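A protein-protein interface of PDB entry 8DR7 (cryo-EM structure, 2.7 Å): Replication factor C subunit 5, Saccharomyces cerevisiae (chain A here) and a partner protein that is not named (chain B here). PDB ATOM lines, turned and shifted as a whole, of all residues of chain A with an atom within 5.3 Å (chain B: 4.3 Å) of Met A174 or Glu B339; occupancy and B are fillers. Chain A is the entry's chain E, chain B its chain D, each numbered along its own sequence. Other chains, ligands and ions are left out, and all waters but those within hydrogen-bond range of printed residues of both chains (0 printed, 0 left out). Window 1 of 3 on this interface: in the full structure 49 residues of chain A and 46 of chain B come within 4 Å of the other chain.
Met A174 touches just these residues of chain B: Ser B296 (3.8 Å) and Glu B339 (3.8 Å).
Glu B339 touches just these residues of chain A: Ser A173 (2.9 Å), Met A174 (3.8 Å) and Ser A175 (3.0 Å).
Of the printed residues of chain B, Ser A175 touches Leu B333, Thr B337 and Glu B339.
Of the printed residues of chain A, Thr B337 touches Ser A175 (3.5 Å).
Leu B343 touches none of the printed residues of chain A.
The nearest printed residue of chain B that does not touch Met A174 is Ala B297 (6.6 Å).
The nearest printed residue of chain A that does not touch Glu B339 is Asp A172 (5.3 Å).
The nearest printed residue of chain A that does not touch Ser B296 is Tyr A42 (4.6 Å).
OE1 of Glu B339 is in hydrogen-bond range of OG of Ser A173 (2.9 Å).
The side-chain carboxylate of Glu B339 is in hydrogen-bond range of the side-chain hydroxyl of Ser A175 (3.0 Å).
The backbone carbonyl oxygen (O) of Met A174 is in hydrogen-bond range of the side-chain amino group (NZ) of Lys A182, 2.8 Å away.
The side-chain sulfur of Cys A171 lies within hydrogen-bond range of the backbone carbonyl oxygen of Ser A173 (3.4 Å).
Hydrophobic or aromatic side chains of chain A within 4 Å of the printed part of chain B: Met A174.
Of the 11 printed residues of chain B, 4 touch a printed residue of chain A.
Among the printed residues, no Asp or Glu carboxylate lies within 4 Å of a Lys or Arg side-chain nitrogen of the other chain.
Among the printed residues, merely in contact across the chains: Ser A175 with Thr B337, Met A174 with Glu B339, Met A174 with Ser B296 and Ser A175 with Leu B333.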
ATOM      1  N   LEU A  40       5.037  15.348   6.765  1.00  0.00           N
ATOM      2  CA  LEU A  40       4.916  14.031   7.379  1.00  0.00           C
ATOM      3  C   LEU A  40       6.023  13.148   6.827  1.00  0.00           C
ATOM      4  O   LEU A  40       5.991  12.769   5.652  1.00  0.00           O
ATOM      5  CB  LEU A  40       3.543  13.413   7.103  1.00  0.00           C
ATOM      6  CG  LEU A  40       3.193  12.182   7.943  1.00  0.00           C
ATOM      7  CD1 LEU A  40       1.710  12.168   8.274  1.00  0.00           C
ATOM      8  CD2 LEU A  40       3.593  10.902   7.224  1.00  0.00           C
ATOM      9  N   TYR A  42       8.003   9.628   6.716  1.00  0.00           N
ATOM     10  CA  TYR A  42       7.804   8.205   6.941  1.00  0.00           C
ATOM     11  C   TYR A  42       8.951   7.414   6.330  1.00  0.00           C
ATOM     12  O   TYR A  42       9.497   7.779   5.284  1.00  0.00           O
ATOM     13  CB  TYR A  42       6.461   7.722   6.365  1.00  0.00           C
ATOM     14  CG  TYR A  42       6.331   7.860   4.866  1.00  0.00           C
ATOM     15  CD1 TYR A  42       5.992   9.076   4.288  1.00  0.00           C
ATOM     16  CD2 TYR A  42       6.533   6.771   4.030  1.00  0.00           C
ATOM     17  CE1 TYR A  42       5.866   9.205   2.920  1.00  0.00           C
ATOM     18  CE2 TYR A  42       6.409   6.891   2.659  1.00  0.00           C
ATOM     19  CZ  TYR A  42       6.074   8.109   2.111  1.00  0.00           C
ATOM     20  OH  TYR A  42       5.950   8.233   0.746  1.00  0.00           O
ATOM     21  N   CYS A 171       6.991   9.366  11.578  1.00  0.00           N
ATOM     22  CA  CYS A 171       6.436   8.061  11.907  1.00  0.00           C
ATOM     23  C   CYS A 171       7.153   6.990  11.100  1.00  0.00           C
ATOM     24  O   CYS A 171       7.763   7.268  10.064  1.00  0.00           O
ATOM     25  CB  CYS A 171       4.927   8.009  11.639  1.00  0.00           C
ATOM     26  SG  CYS A 171       4.480   8.026   9.888  1.00  0.00           S
ATOM     27  N   ASP A 172       7.080   5.755  11.595  1.00  0.00           N
ATOM     28  CA  ASP A 172       7.677   4.614  10.914  1.00  0.00           C
ATOM     29  C   ASP A 172       6.699   3.883  10.004  1.00  0.00           C
ATOM     30  O   ASP A 172       7.123   3.002   9.248  1.00  0.00           O
ATOM     31  CB  ASP A 172       8.248   3.624  11.937  1.00  0.00           C
ATOM     32  CG  ASP A 172       7.232   3.212  12.985  1.00  0.00           C
ATOM     33  OD1 ASP A 172       6.048   3.585  12.848  1.00  0.00           O
ATOM     34  OD2 ASP A 172       7.618   2.514  13.945  1.00  0.00           O
ATOM     35  N   SER A 173       5.413   4.221  10.055  1.00  0.00           N
ATOM     36  CA  SER A 173       4.416   3.579   9.211  1.00  0.00           C
ATOM     37  C   SER A 173       3.184   4.471   9.151  1.00  0.00           C
ATOM     38  O   SER A 173       2.796   5.068  10.158  1.00  0.00           O
ATOM     39  CB  SER A 173       4.044   2.190   9.742  1.00  0.00           C
ATOM     40  OG  SER A 173       3.457   1.396   8.726  1.00  0.00           O
ATOM     41  N   MET A 174       2.579   4.555   7.968  1.00  0.00           N
ATOM     42  CA  MET A 174       1.414   5.398   7.744  1.00  0.00           C
ATOM     43  C   MET A 174       0.096   4.648   7.879  1.00  0.00           C
ATOM     44  O   MET A 174      -0.965   5.262   7.730  1.00  0.00           O
ATOM     45  CB  MET A 174       1.493   6.038   6.354  1.00  0.00           C
ATOM     46  CG  MET A 174       2.126   7.422   6.346  1.00  0.00           C
ATOM     47  SD  MET A 174       2.163   8.204   4.717  1.00  0.00           S
ATOM     48  CE  MET A 174       2.696   6.850   3.671  1.00  0.00           C
ATOM     49  N   SER A 175       0.130   3.344   8.157  1.00  0.00           N
ATOM     50  CA  SER A 175      -1.114   2.582   8.231  1.00  0.00           C
ATOM     51  C   SER A 175      -2.044   3.095   9.323  1.00  0.00           C
ATOM     52  O   SER A 175      -3.241   3.281   9.046  1.00  0.00           O
ATOM     53  CB  SER A 175      -0.797   1.094   8.417  1.00  0.00           C
ATOM     54  OG  SER A 175       0.043   0.621   7.380  1.00  0.00           O
ATOM     55  N   PRO A 176      -1.589   3.340  10.558  1.00  0.00           N
ATOM     56  CA  PRO A 176      -2.509   3.876  11.575  1.00  0.00           C
ATOM     57  C   PRO A 176      -3.004   5.279  11.269  1.00  0.00           C
ATOM     58  O   PRO A 176      -4.030   5.689  11.827  1.00  0.00           O
ATOM     59  CB  PRO A 176      -1.670   3.849  12.861  1.00  0.00           C
ATOM     60  CG  PRO A 176      -0.532   2.919  12.568  1.00  0.00           C
ATOM     61  CD  PRO A 176      -0.248   3.110  11.117  1.00  0.00           C
ATOM     62  N   ILE A 177      -2.314   6.026  10.406  1.00  0.00           N
ATOM     63  CA  ILE A 177      -2.707   7.399  10.114  1.00  0.00           C
ATOM     64  C   ILE A 177      -3.983   7.402   9.282  1.00  0.00           C
ATOM     65  O   ILE A 177      -4.135   6.616   8.338  1.00  0.00           O
ATOM     66  CB  ILE A 177      -1.570   8.144   9.392  1.00  0.00           C
ATOM     67  CG1 ILE A 177      -0.241   7.977  10.139  1.00  0.00           C
ATOM     68  CG2 ILE A 177      -1.917   9.618   9.230  1.00  0.00           C
ATOM     69  CD1 ILE A 177      -0.182   8.699  11.470  1.00  0.00           C
ATOM     70  N   LYS A 182      -3.422  12.379   6.295  1.00  0.00           N
ATOM     71  CA  LYS A 182      -2.536  12.209   5.148  1.00  0.00           C
ATOM     72  C   LYS A 182      -2.801  13.278   4.097  1.00  0.00           C
ATOM     73  O   LYS A 182      -1.863  13.807   3.486  1.00  0.00           O
ATOM     74  CB  LYS A 182      -2.718  10.816   4.544  1.00  0.00           C
ATOM     75  CG  LYS A 182      -1.478   9.940   4.610  1.00  0.00           C
ATOM     76  CD  LYS A 182      -1.825   8.474   4.404  1.00  0.00           C
ATOM     77  CE  LYS A 182      -2.423   7.860   5.658  1.00  0.00           C
ATOM     78  NZ  LYS A 182      -2.466   6.373   5.595  1.00  0.00           N
ATOM     79  N   LEU A 187       3.777  14.448   2.101  1.00  0.00           N
ATOM     80  CA  LEU A 187       4.426  13.165   2.341  1.00  0.00           C
ATOM     81  C   LEU A 187       5.902  13.254   1.971  1.00  0.00           C
ATOM     82  O   LEU A 187       6.247  13.748   0.893  1.00  0.00           O
ATOM     83  CB  LEU A 187       3.738  12.069   1.529  1.00  0.00           C
ATOM     84  CG  LEU A 187       2.566  11.337   2.190  1.00  0.00           C
ATOM     85  CD1 LEU A 187       1.646  12.307   2.914  1.00  0.00           C
ATOM     86  CD2 LEU A 187       1.791  10.544   1.149  1.00  0.00           C
ATOM     87  N   MET B 291      11.221  -3.532   1.553  1.00  0.00           N
ATOM     88  CA  MET B 291      10.675  -2.758   2.663  1.00  0.00           C
ATOM     89  C   MET B 291      11.679  -1.779   3.255  1.00  0.00           C
ATOM     90  O   MET B 291      11.279  -0.917   4.045  1.00  0.00           O
ATOM     91  CB  MET B 291      10.166  -3.696   3.759  1.00  0.00           C
ATOM     92  CG  MET B 291       9.004  -4.581   3.329  1.00  0.00           C
ATOM     93  SD  MET B 291       7.467  -3.677   3.040  1.00  0.00           S
ATOM     94  CE  MET B 291       7.213  -2.879   4.624  1.00  0.00           C
ATOM     95  N   SER B 296       5.110   2.906   0.692  1.00  0.00           N
ATOM     96  CA  SER B 296       3.874   2.628   1.408  1.00  0.00           C
ATOM     97  C   SER B 296       3.204   1.380   0.849  1.00  0.00           C
ATOM     98  O   SER B 296       3.193   1.151  -0.364  1.00  0.00           O
ATOM     99  CB  SER B 296       2.925   3.822   1.313  1.00  0.00           C
ATOM    100  OG  SER B 296       2.361   3.922   0.017  1.00  0.00           O
ATOM    101  N   ALA B 297       2.639   0.568   1.746  1.00  0.00           N
ATOM    102  CA  ALA B 297       2.005  -0.675   1.320  1.00  0.00           C
ATOM    103  C   ALA B 297       0.757  -0.410   0.488  1.00  0.00           C
ATOM    104  O   ALA B 297       0.455  -1.165  -0.443  1.00  0.00           O
ATOM    105  CB  ALA B 297       1.661  -1.532   2.537  1.00  0.00           C
ATOM    106  N   LEU B 333      -4.983  -3.759   5.995  1.00  0.00           N
ATOM    107  CA  LEU B 333      -4.064  -2.631   6.096  1.00  0.00           C
ATOM    108  C   LEU B 333      -4.766  -1.376   6.598  1.00  0.00           C
ATOM    109  O   LEU B 333      -4.149  -0.558   7.289  1.00  0.00           O
ATOM    110  CB  LEU B 333      -3.411  -2.362   4.740  1.00  0.00           C
ATOM    111  CG  LEU B 333      -2.141  -3.159   4.435  1.00  0.00           C
ATOM    112  CD1 LEU B 333      -1.771  -3.030   2.966  1.00  0.00           C
ATOM    113  CD2 LEU B 333      -0.989  -2.701   5.317  1.00  0.00           C
ATOM    114  N   THR B 337      -2.033  -2.013  10.600  1.00  0.00           N
ATOM    115  CA  THR B 337      -1.229  -3.188  10.908  1.00  0.00           C
ATOM    116  C   THR B 337       0.158  -3.042  10.288  1.00  0.00           C
ATOM    117  O   THR B 337       0.446  -2.087   9.561  1.00  0.00           O
ATOM    118  CB  THR B 337      -1.920  -4.459  10.406  1.00  0.00           C
ATOM    119  OG1 THR B 337      -2.155  -4.354   8.996  1.00  0.00           O
ATOM    120  CG2 THR B 337      -3.244  -4.666  11.124  1.00  0.00           C
ATOM    121  N   ASN B 338       1.024  -4.007  10.586  1.00  0.00           N
ATOM    122  CA  ASN B 338       2.376  -3.990  10.043  1.00  0.00           C
ATOM    123  C   ASN B 338       2.333  -4.228   8.539  1.00  0.00           C
ATOM    124  O   ASN B 338       1.681  -5.163   8.065  1.00  0.00           O
ATOM    125  CB  ASN B 338       3.236  -5.051  10.730  1.00  0.00           C
ATOM    126  CG  ASN B 338       4.636  -5.134  10.153  1.00  0.00           C
ATOM    127  OD1 ASN B 338       4.824  -5.502   8.993  1.00  0.00           O
ATOM    128  ND2 ASN B 338       5.630  -4.792  10.964  1.00  0.00           N
ATOM    129  N   GLU B 339       3.035  -3.379   7.787  1.00  0.00           N
ATOM    130  CA  GLU B 339       2.992  -3.469   6.332  1.00  0.00           C
ATOM    131  C   GLU B 339       3.798  -4.652   5.811  1.00  0.00           C
ATOM    132  O   GLU B 339       3.406  -5.277   4.819  1.00  0.00           O
ATOM    133  CB  GLU B 339       3.506  -2.169   5.718  1.00  0.00           C
ATOM    134  CG  GLU B 339       2.567  -0.986   5.903  1.00  0.00           C
ATOM    135  CD  GLU B 339       3.270   0.352   5.771  1.00  0.00           C
ATOM    136  OE1 GLU B 339       2.603   1.393   5.942  1.00  0.00           O
ATOM    137  OE2 GLU B 339       4.488   0.363   5.495  1.00  0.00           O
ATOM    138  N   HIS B 340       4.920  -4.971   6.459  1.00  0.00           N
ATOM    139  CA  HIS B 340       5.781  -6.046   5.973  1.00  0.00           C
ATOM    140  C   HIS B 340       5.035  -7.375   5.939  1.00  0.00           C
ATOM    141  O   HIS B 340       5.040  -8.079   4.921  1.00  0.00           O
ATOM    142  CB  HIS B 340       7.022  -6.147   6.861  1.00  0.00           C
ATOM    143  CG  HIS B 340       8.162  -6.885   6.230  1.00  0.00           C
ATOM    144  ND1 HIS B 340       9.479  -6.540   6.446  1.00  0.00           N
ATOM    145  CD2 HIS B 340       8.184  -7.949   5.393  1.00  0.00           C
ATOM    146  CE1 HIS B 340      10.263  -7.360   5.770  1.00  0.00           C
ATOM    147  NE2 HIS B 340       9.503  -8.225   5.122  1.00  0.00           N
ATOM    148  N   ILE B 341       4.385  -7.732   7.048  1.00  0.00           N
ATOM    149  CA  ILE B 341       3.714  -9.027   7.137  1.00  0.00           C
ATOM    150  C   ILE B 341       2.578  -9.106   6.127  1.00  0.00           C
ATOM    151  O   ILE B 341       2.410 -10.115   5.431  1.00  0.00           O
ATOM    152  CB  ILE B 341       3.210  -9.270   8.572  1.00  0.00           C
ATOM    153  CG1 ILE B 341       4.392  -9.360   9.542  1.00  0.00           C
ATOM    154  CG2 ILE B 341       2.370 -10.539   8.633  1.00  0.00           C
ATOM    155  CD1 ILE B 341       3.995  -9.291  11.002  1.00  0.00           C
ATOM    156  N   GLN B 342       1.772  -8.046   6.039  1.00  0.00           N
ATOM    157  CA  GLN B 342       0.642  -8.056   5.116  1.00  0.00           C
ATOM    158  C   GLN B 342       1.111  -8.165   3.672  1.00  0.00           C
ATOM    159  O   GLN B 342       0.542  -8.931   2.883  1.00  0.00           O
ATOM    160  CB  GLN B 342      -0.204  -6.797   5.311  1.00  0.00           C
ATOM    161  CG  GLN B 342      -0.798  -6.655   6.703  1.00  0.00           C
ATOM    162  CD  GLN B 342      -1.774  -7.764   7.040  1.00  0.00           C
ATOM    163  OE1 GLN B 342      -2.419  -8.329   6.157  1.00  0.00           O
ATOM    164  NE2 GLN B 342      -1.889  -8.082   8.324  1.00  0.00           N
ATOM    165  N   LEU B 343       2.148  -7.410   3.305  1.00  0.00           N
ATOM    166  CA  LEU B 343       2.653  -7.470   1.938  1.00  0.00           C
ATOM    167  C   LEU B 343       3.213  -8.850   1.620  1.00  0.00           C
ATOM    168  O   LEU B 343       2.962  -9.396   0.537  1.00  0.00           O
ATOM    169  CB  LEU B 343       3.722  -6.397   1.728  1.00  0.00           C
ATOM    170  CG  LEU B 343       4.229  -6.222   0.294  1.00  0.00           C
ATOM    171  CD1 LEU B 343       3.099  -5.806  -0.637  1.00  0.00           C
ATOM    172  CD2 LEU B 343       5.362  -5.210   0.249  1.00  0.00           C
